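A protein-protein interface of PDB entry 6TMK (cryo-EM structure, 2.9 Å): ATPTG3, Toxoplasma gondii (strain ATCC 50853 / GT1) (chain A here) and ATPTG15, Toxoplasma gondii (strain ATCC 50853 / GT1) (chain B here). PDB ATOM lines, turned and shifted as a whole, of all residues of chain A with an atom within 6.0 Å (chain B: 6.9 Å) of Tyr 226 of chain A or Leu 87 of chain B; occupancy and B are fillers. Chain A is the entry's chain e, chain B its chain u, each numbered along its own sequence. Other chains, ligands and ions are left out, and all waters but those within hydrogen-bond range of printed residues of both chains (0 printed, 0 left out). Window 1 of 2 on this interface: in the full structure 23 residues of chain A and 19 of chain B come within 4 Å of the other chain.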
ATOM      1  N   PRO A 217      22.919  24.225  -8.075  1.00  0.00           N
ATOM      2  CA  PRO A 217      21.815  24.024  -7.129  1.00  0.00           C
ATOM      3  C   PRO A 217      21.879  22.705  -6.395  1.00  0.00           C
ATOM      4  O   PRO A 217      21.434  22.634  -5.245  1.00  0.00           O
ATOM      5  CB  PRO A 217      20.571  24.119  -8.019  1.00  0.00           C
ATOM      6  CG  PRO A 217      21.024  24.830  -9.221  1.00  0.00           C
ATOM      7  CD  PRO A 217      22.416  24.389  -9.443  1.00  0.00           C
ATOM      8  N   PHE A 218      22.398  21.656  -7.017  1.00  0.00           N
ATOM      9  CA  PHE A 218      22.517  20.388  -6.323  1.00  0.00           C
ATOM     10  C   PHE A 218      23.590  20.488  -5.246  1.00  0.00           C
ATOM     11  O   PHE A 218      24.560  21.240  -5.366  1.00  0.00           O
ATOM     12  CB  PHE A 218      22.845  19.268  -7.303  1.00  0.00           C
ATOM     13  CG  PHE A 218      22.438  17.915  -6.824  1.00  0.00           C
ATOM     14  CD1 PHE A 218      21.115  17.527  -6.842  1.00  0.00           C
ATOM     15  CD2 PHE A 218      23.380  17.031  -6.346  1.00  0.00           C
ATOM     16  CE1 PHE A 218      20.744  16.284  -6.394  1.00  0.00           C
ATOM     17  CE2 PHE A 218      23.016  15.794  -5.898  1.00  0.00           C
ATOM     18  CZ  PHE A 218      21.697  15.415  -5.924  1.00  0.00           C
ATOM     19  N   VAL A 219      23.407  19.711  -4.186  1.00  0.00           N
ATOM     20  CA  VAL A 219      24.242  19.772  -2.995  1.00  0.00           C
ATOM     21  C   VAL A 219      24.819  18.386  -2.756  1.00  0.00           C
ATOM     22  O   VAL A 219      24.076  17.433  -2.492  1.00  0.00           O
ATOM     23  CB  VAL A 219      23.454  20.264  -1.771  1.00  0.00           C
ATOM     24  CG1 VAL A 219      24.279  20.140  -0.525  1.00  0.00           C
ATOM     25  CG2 VAL A 219      23.009  21.691  -1.961  1.00  0.00           C
ATOM     26  N   SER A 221      27.079  17.884  -0.327  1.00  0.00           N
ATOM     27  CA  SER A 221      27.621  17.919   1.020  1.00  0.00           C
ATOM     28  C   SER A 221      26.859  17.032   1.994  1.00  0.00           C
ATOM     29  O   SER A 221      27.139  17.080   3.195  1.00  0.00           O
ATOM     30  CB  SER A 221      27.632  19.355   1.539  1.00  0.00           C
ATOM     31  OG  SER A 221      28.642  20.116   0.903  1.00  0.00           O
ATOM     32  N   SER A 222      25.911  16.231   1.517  1.00  0.00           N
ATOM     33  CA  SER A 222      25.269  15.235   2.355  1.00  0.00           C
ATOM     34  C   SER A 222      24.815  14.075   1.488  1.00  0.00           C
ATOM     35  O   SER A 222      24.846  14.137   0.258  1.00  0.00           O
ATOM     36  CB  SER A 222      24.083  15.823   3.120  1.00  0.00           C
ATOM     37  OG  SER A 222      23.564  14.891   4.044  1.00  0.00           O
ATOM     38  N   SER A 224      21.674  12.650   1.681  1.00  0.00           N
ATOM     39  CA  SER A 224      20.299  12.842   1.271  1.00  0.00           C
ATOM     40  C   SER A 224      20.194  14.018   0.303  1.00  0.00           C
ATOM     41  O   SER A 224      20.996  14.952   0.362  1.00  0.00           O
ATOM     42  CB  SER A 224      19.417  13.079   2.490  1.00  0.00           C
ATOM     43  OG  SER A 224      19.745  14.288   3.143  1.00  0.00           O
ATOM     44  N   PRO A 225      19.212  14.000  -0.600  1.00  0.00           N
ATOM     45  CA  PRO A 225      19.168  15.021  -1.653  1.00  0.00           C
ATOM     46  C   PRO A 225      18.747  16.381  -1.119  1.00  0.00           C
ATOM     47  O   PRO A 225      17.702  16.526  -0.478  1.00  0.00           O
ATOM     48  CB  PRO A 225      18.142  14.465  -2.647  1.00  0.00           C
ATOM     49  CG  PRO A 225      17.873  13.070  -2.220  1.00  0.00           C
ATOM     50  CD  PRO A 225      18.125  13.027  -0.760  1.00  0.00           C
ATOM     51  N   TYR A 226      19.563  17.384  -1.426  1.00  0.00           N
ATOM     52  CA  TYR A 226      19.274  18.775  -1.130  1.00  0.00           C
ATOM     53  C   TYR A 226      19.369  19.593  -2.409  1.00  0.00           C
ATOM     54  O   TYR A 226      20.189  19.312  -3.285  1.00  0.00           O
ATOM     55  CB  TYR A 226      20.249  19.341  -0.094  1.00  0.00           C
ATOM     56  CG  TYR A 226      19.974  18.979   1.343  1.00  0.00           C
ATOM     57  CD1 TYR A 226      19.377  19.882   2.197  1.00  0.00           C
ATOM     58  CD2 TYR A 226      20.352  17.754   1.858  1.00  0.00           C
ATOM     59  CE1 TYR A 226      19.137  19.571   3.507  1.00  0.00           C
ATOM     60  CE2 TYR A 226      20.117  17.434   3.172  1.00  0.00           C
ATOM     61  CZ  TYR A 226      19.511  18.346   3.993  1.00  0.00           C
ATOM     62  OH  TYR A 226      19.271  18.034   5.311  1.00  0.00           O
ATOM     63  N   ILE A 227      18.517  20.606  -2.510  1.00  0.00           N
ATOM     64  CA  ILE A 227      18.505  21.521  -3.643  1.00  0.00           C
ATOM     65  C   ILE A 227      18.537  22.942  -3.105  1.00  0.00           C
ATOM     66  O   ILE A 227      17.863  23.255  -2.120  1.00  0.00           O
ATOM     67  CB  ILE A 227      17.269  21.308  -4.541  1.00  0.00           C
ATOM     68  CG1 ILE A 227      17.391  20.011  -5.339  1.00  0.00           C
ATOM     69  CG2 ILE A 227      17.098  22.460  -5.485  1.00  0.00           C
ATOM     70  CD1 ILE A 227      18.282  20.106  -6.541  1.00  0.00           C
ATOM     71  N   ARG A 228      19.328  23.801  -3.734  1.00  0.00           N
ATOM     72  CA  ARG A 228      19.440  25.173  -3.271  1.00  0.00           C
ATOM     73  C   ARG A 228      18.270  26.014  -3.757  1.00  0.00           C
ATOM     74  O   ARG A 228      17.856  25.927  -4.915  1.00  0.00           O
ATOM     75  CB  ARG A 228      20.745  25.803  -3.740  1.00  0.00           C
ATOM     76  CG  ARG A 228      21.974  25.177  -3.160  1.00  0.00           C
ATOM     77  CD  ARG A 228      23.221  25.778  -3.742  1.00  0.00           C
ATOM     78  NE  ARG A 228      24.417  25.075  -3.311  1.00  0.00           N
ATOM     79  CZ  ARG A 228      24.942  25.175  -2.100  1.00  0.00           C
ATOM     80  NH1 ARG A 228      24.377  25.950  -1.190  1.00  0.00           N
ATOM     81  NH2 ARG A 228      26.033  24.498  -1.798  1.00  0.00           N
ATOM     82  N   PRO A 239      19.924  25.504   1.333  1.00  0.00           N
ATOM     83  CA  PRO A 239      19.576  24.152   0.886  1.00  0.00           C
ATOM     84  C   PRO A 239      18.293  23.648   1.522  1.00  0.00           C
ATOM     85  O   PRO A 239      18.029  23.862   2.706  1.00  0.00           O
ATOM     86  CB  PRO A 239      20.781  23.308   1.323  1.00  0.00           C
ATOM     87  CG  PRO A 239      21.824  24.270   1.728  1.00  0.00           C
ATOM     88  CD  PRO A 239      21.126  25.492   2.177  1.00  0.00           C
ATOM     89  N   VAL A 240      17.499  22.964   0.706  1.00  0.00           N
ATOM     90  CA  VAL A 240      16.197  22.434   1.082  1.00  0.00           C
ATOM     91  C   VAL A 240      16.202  20.945   0.772  1.00  0.00           C
ATOM     92  O   VAL A 240      16.568  20.554  -0.345  1.00  0.00           O
ATOM     93  CB  VAL A 240      15.069  23.152   0.330  1.00  0.00           C
ATOM     94  CG1 VAL A 240      13.731  22.824   0.936  1.00  0.00           C
ATOM     95  CG2 VAL A 240      15.303  24.640   0.329  1.00  0.00           C
ATOM     96  N   PRO A 241      15.830  20.083   1.709  1.00  0.00           N
ATOM     97  CA  PRO A 241      15.824  18.651   1.420  1.00  0.00           C
ATOM     98  C   PRO A 241      14.629  18.249   0.577  1.00  0.00           C
ATOM     99  O   PRO A 241      13.536  18.807   0.684  1.00  0.00           O
ATOM    100  CB  PRO A 241      15.760  18.021   2.815  1.00  0.00           C
ATOM    101  CG  PRO A 241      15.035  19.011   3.614  1.00  0.00           C
ATOM    102  CD  PRO A 241      15.446  20.351   3.103  1.00  0.00           C
ATOM    103  N   LEU A 242      14.857  17.254  -0.274  1.00  0.00           N
ATOM    104  CA  LEU A 242      13.831  16.790  -1.194  1.00  0.00           C
ATOM    105  C   LEU A 242      13.065  15.583  -0.688  1.00  0.00           C
ATOM    106  O   LEU A 242      11.877  15.445  -0.992  1.00  0.00           O
ATOM    107  CB  LEU A 242      14.452  16.436  -2.543  1.00  0.00           C
ATOM    108  CG  LEU A 242      15.233  17.527  -3.252  1.00  0.00           C
ATOM    109  CD1 LEU A 242      15.953  16.931  -4.425  1.00  0.00           C
ATOM    110  CD2 LEU A 242      14.307  18.626  -3.701  1.00  0.00           C
ATOM    111  N   ALA B  82      31.341  24.344   6.401  1.00  0.00           N
ATOM    112  CA  ALA B  82      30.203  24.849   7.154  1.00  0.00           C
ATOM    113  C   ALA B  82      28.896  24.271   6.637  1.00  0.00           C
ATOM    114  O   ALA B  82      27.979  24.002   7.417  1.00  0.00           O
ATOM    115  CB  ALA B  82      30.182  26.370   7.080  1.00  0.00           C
ATOM    116  N   GLU B  83      28.782  24.099   5.324  1.00  0.00           N
ATOM    117  CA  GLU B  83      27.577  23.510   4.756  1.00  0.00           C
ATOM    118  C   GLU B  83      27.381  22.085   5.252  1.00  0.00           C
ATOM    119  O   GLU B  83      26.276  21.693   5.652  1.00  0.00           O
ATOM    120  CB  GLU B  83      27.656  23.538   3.238  1.00  0.00           C
ATOM    121  CG  GLU B  83      26.320  23.442   2.560  1.00  0.00           C
ATOM    122  CD  GLU B  83      26.443  23.089   1.101  1.00  0.00           C
ATOM    123  OE1 GLU B  83      27.554  23.223   0.550  1.00  0.00           O
ATOM    124  OE2 GLU B  83      25.433  22.671   0.503  1.00  0.00           O
ATOM    125  N   LYS B  84      28.448  21.286   5.205  1.00  0.00           N
ATOM    126  CA  LYS B  84      28.370  19.925   5.726  1.00  0.00           C
ATOM    127  C   LYS B  84      27.932  19.920   7.185  1.00  0.00           C
ATOM    128  O   LYS B  84      27.063  19.136   7.587  1.00  0.00           O
ATOM    129  CB  LYS B  84      29.722  19.245   5.564  1.00  0.00           C
ATOM    130  CG  LYS B  84      30.053  18.907   4.158  1.00  0.00           C
ATOM    131  CD  LYS B  84      31.426  18.320   4.034  1.00  0.00           C
ATOM    132  CE  LYS B  84      31.796  18.111   2.584  1.00  0.00           C
ATOM    133  NZ  LYS B  84      32.568  19.256   2.032  1.00  0.00           N
ATOM    134  N   GLN B  85      28.527  20.798   7.988  1.00  0.00           N
ATOM    135  CA  GLN B  85      28.191  20.889   9.403  1.00  0.00           C
ATOM    136  C   GLN B  85      26.721  21.239   9.600  1.00  0.00           C
ATOM    137  O   GLN B  85      26.021  20.637  10.427  1.00  0.00           O
ATOM    138  CB  GLN B  85      29.101  21.925  10.047  1.00  0.00           C
ATOM    139  CG  GLN B  85      28.856  22.210  11.478  1.00  0.00           C
ATOM    140  CD  GLN B  85      29.919  23.098  12.053  1.00  0.00           C
ATOM    141  OE1 GLN B  85      30.809  23.558  11.344  1.00  0.00           O
ATOM    142  NE2 GLN B  85      29.838  23.351  13.337  1.00  0.00           N
ATOM    143  N   LYS B  86      26.244  22.223   8.843  1.00  0.00           N
ATOM    144  CA  LYS B  86      24.857  22.652   8.918  1.00  0.00           C
ATOM    145  C   LYS B  86      23.913  21.497   8.636  1.00  0.00           C
ATOM    146  O   LYS B  86      22.950  21.268   9.378  1.00  0.00           O
ATOM    147  CB  LYS B  86      24.633  23.774   7.913  1.00  0.00           C
ATOM    148  CG  LYS B  86      23.333  24.506   8.042  1.00  0.00           C
ATOM    149  CD  LYS B  86      22.932  25.111   6.723  1.00  0.00           C
ATOM    150  CE  LYS B  86      23.781  26.306   6.377  1.00  0.00           C
ATOM    151  NZ  LYS B  86      23.837  26.498   4.908  1.00  0.00           N
ATOM    152  N   LEU B  87      24.162  20.770   7.550  1.00  0.00           N
ATOM    153  CA  LEU B  87      23.247  19.705   7.168  1.00  0.00           C
ATOM    154  C   LEU B  87      23.286  18.561   8.170  1.00  0.00           C
ATOM    155  O   LEU B  87      22.249  17.950   8.462  1.00  0.00           O
ATOM    156  CB  LEU B  87      23.580  19.225   5.764  1.00  0.00           C
ATOM    157  CG  LEU B  87      23.513  20.293   4.678  1.00  0.00           C
ATOM    158  CD1 LEU B  87      23.673  19.652   3.338  1.00  0.00           C
ATOM    159  CD2 LEU B  87      22.232  21.085   4.732  1.00  0.00           C
ATOM    160  N   PHE B  88      24.461  18.274   8.729  1.00  0.00           N
ATOM    161  CA  PHE B  88      24.542  17.277   9.786  1.00  0.00           C
ATOM    162  C   PHE B  88      23.657  17.651  10.966  1.00  0.00           C
ATOM    163  O   PHE B  88      22.850  16.841  11.440  1.00  0.00           O
ATOM    164  CB  PHE B  88      25.989  17.118  10.247  1.00  0.00           C
ATOM    165  CG  PHE B  88      26.145  16.168  11.382  1.00  0.00           C
ATOM    166  CD1 PHE B  88      26.299  14.824  11.155  1.00  0.00           C
ATOM    167  CD2 PHE B  88      26.111  16.618  12.682  1.00  0.00           C
ATOM    168  CE1 PHE B  88      26.426  13.953  12.199  1.00  0.00           C
ATOM    169  CE2 PHE B  88      26.235  15.751  13.720  1.00  0.00           C
ATOM    170  CZ  PHE B  88      26.387  14.418  13.482  1.00  0.00           C
ATOM    171  N   HIS B  89      23.820  18.874  11.474  1.00  0.00           N
ATOM    172  CA  HIS B  89      23.036  19.303  12.627  1.00  0.00           C
ATOM    173  C   HIS B  89      21.545  19.285  12.327  1.00  0.00           C
ATOM    174  O   HIS B  89      20.731  18.890  13.172  1.00  0.00           O
ATOM    175  CB  HIS B  89      23.484  20.696  13.052  1.00  0.00           C
ATOM    176  CG  HIS B  89      24.708  20.702  13.908  1.00  0.00           C
ATOM    177  ND1 HIS B  89      25.712  21.632  13.761  1.00  0.00           N
ATOM    178  CD2 HIS B  89      25.074  19.914  14.944  1.00  0.00           C
ATOM    179  CE1 HIS B  89      26.657  21.401  14.652  1.00  0.00           C
ATOM    180  NE2 HIS B  89      26.294  20.365  15.384  1.00  0.00           N
ATOM    181  N   GLN B  90      21.173  19.704  11.121  1.00  0.00           N
ATOM    182  CA  GLN B  90      19.777  19.675  10.710  1.00  0.00           C
ATOM    183  C   GLN B  90      19.209  18.262  10.789  1.00  0.00           C
ATOM    184  O   GLN B  90      18.166  18.027  11.416  1.00  0.00           O
ATOM    185  CB  GLN B  90      19.681  20.233   9.297  1.00  0.00           C
ATOM    186  CG  GLN B  90      18.362  20.793   8.906  1.00  0.00           C
ATOM    187  CD  GLN B  90      18.463  21.645   7.668  1.00  0.00           C
ATOM    188  OE1 GLN B  90      19.255  22.584   7.611  1.00  0.00           O
ATOM    189  NE2 GLN B  90      17.685  21.304   6.652  1.00  0.00           N
ATOM    190  N   GLU B  91      19.879  17.310  10.138  1.00  0.00           N
ATOM    191  CA  GLU B  91      19.402  15.934  10.131  1.00  0.00           C
ATOM    192  C   GLU B  91      19.303  15.373  11.543  1.00  0.00           C
ATOM    193  O   GLU B  91      18.348  14.655  11.873  1.00  0.00           O
ATOM    194  CB  GLU B  91      20.330  15.084   9.270  1.00  0.00           C
ATOM    195  CG  GLU B  91      20.229  15.392   7.792  1.00  0.00           C
ATOM    196  CD  GLU B  91      21.527  15.157   7.049  1.00  0.00           C
ATOM    197  OE1 GLU B  91      22.378  14.396   7.556  1.00  0.00           O
ATOM    198  OE2 GLU B  91      21.700  15.738   5.959  1.00  0.00           O
ATOM    199  N   LEU B  92      20.283  15.684  12.391  1.00  0.00           N
ATOM    200  CA  LEU B  92      20.274  15.183  13.761  1.00  0.00           C
ATOM    201  C   LEU B  92      19.065  15.697  14.532  1.00  0.00           C
ATOM    202  O   LEU B  92      18.371  14.933  15.220  1.00  0.00           O
ATOM    203  CB  LEU B  92      21.568  15.597  14.452  1.00  0.00           C
ATOM    204  CG  LEU B  92      21.817  15.072  15.857  1.00  0.00           C
ATOM    205  CD1 LEU B  92      22.445  13.713  15.799  1.00  0.00           C
ATOM    206  CD2 LEU B  92      22.695  16.029  16.619  1.00  0.00           C
ATOM    207  N   ARG B  94      16.263  16.727  13.327  1.00  0.00           N
ATOM    208  CA  ARG B  94      15.069  16.098  12.778  1.00  0.00           C
ATOM    209  C   ARG B  94      14.875  14.700  13.344  1.00  0.00           C
ATOM    210  O   ARG B  94      13.755  14.317  13.701  1.00  0.00           O
ATOM    211  CB  ARG B  94      15.178  16.009  11.263  1.00  0.00           C
ATOM    212  CG  ARG B  94      15.444  17.298  10.541  1.00  0.00           C
ATOM    213  CD  ARG B  94      14.216  17.921   9.981  1.00  0.00           C
ATOM    214  NE  ARG B  94      14.539  19.136   9.241  1.00  0.00           N
ATOM    215  CZ  ARG B  94      14.862  20.290   9.808  1.00  0.00           C
ATOM    216  NH1 ARG B  94      15.140  21.338   9.052  1.00  0.00           N
ATOM    217  NH2 ARG B  94      14.932  20.387  11.124  1.00  0.00           N
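The side-chain carboxylate of Glu 83 of chain B is in hydrogen-bond range of the side-chain hydroxyl of Ser 221 of chain A, 3.3 Å away.
The side-chain carboxylate (OE2) of Glu 91 of chain B sits at hydrogen-bond distance from the side-chain hydroxyl (OH) of Tyr 226 of chain A, 3.4 Å away.
The side-chain hydroxyl of Ser 222 of chain A sits at hydrogen-bond distance from the side-chain carboxylate of Glu 91 of chain B (2.8 Å).
The side-chain carboxylate of Glu 83 of chain B lies within salt-bridge range of the guanidinium group of Arg 228 of chain A, 3.0 Å away.
O of Tyr 226 of chain A lies within hydrogen-bond range of N of Val 219 of chain A (3.4 Å).
The backbone NH of Arg 228 of chain A sits at hydrogen-bond distance from the backbone carbonyl oxygen of Pro 217 of chain A (2.8 Å).
NE2 of Gln 90 of chain B lies close to NH1 of Arg 94 of chain B.
Val 219 of chain A touches Glu 83 of chain B (CG1 to OE2, 3.0 Å).
Leu 87 of chain B touches Val 219 of chain A.
Ser 221 of chain A touches Lys 84 of chain B.
Ser 222 of chain A touches Leu 87 of chain B (CB to CD1, 3.9 Å).
OG of Ser 224 of chain A touches OE2 of Glu 91 of chain B, 3.7 Å away.
Tyr 226 of chain A touches Leu 87 of chain B.
Tyr 226 of chain A touches Gln 90 of chain B.
Pro 239 of chain A touches Lys 86 of chain B (CD to NZ, 3.98 Å).
Of chain B, only Leu 87 (3.7 Å), Gln 90 (3.9 Å) and Glu 91 (3.4 Å) come within 4 Å of Tyr 226 of chain A.
Leu 87 of chain B touches three residues of chain A.
Of the printed residues of chain B, Pro 239 of chain A touches Lys 86 (3.98 Å).
Printed residues of chain A within 4 Å of Gln 90 of chain B: Tyr 226.
Of the printed residues of chain A, Lys 84 of chain B touches Ser 221.
Of the printed residues of chain A, Glu 83 of chain B touches Val 219 (3.0 Å), Ser 221 (3.3 Å) and Arg 228 (3.0 Å).
The nearest printed residue of chain B that does not touch Tyr 226 of chain A is Glu 83 of chain B (6.2 Å).
The nearest printed residue of chain A that does not touch Leu 87 of chain B is Ser 221 of chain A (4.3 Å).
Printed residues of chain B that touch a printed residue of chain A: Glu 83, Lys 84, Lys 86, Leu 87, Gln 90 and Glu 91.
Hydrophobic or aromatic side chains of chain B within 4 Å of the printed part of chain A: Leu 87.
Hydrophobic or aromatic side chains of chain A that line the printed part of chain B: Val 219, Tyr 226 and Pro 239.
Along chain A the printed residues that touch a printed residue of chain B span positions 219 to 239.
Among the printed residues, 12 pairs touch across the chains.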
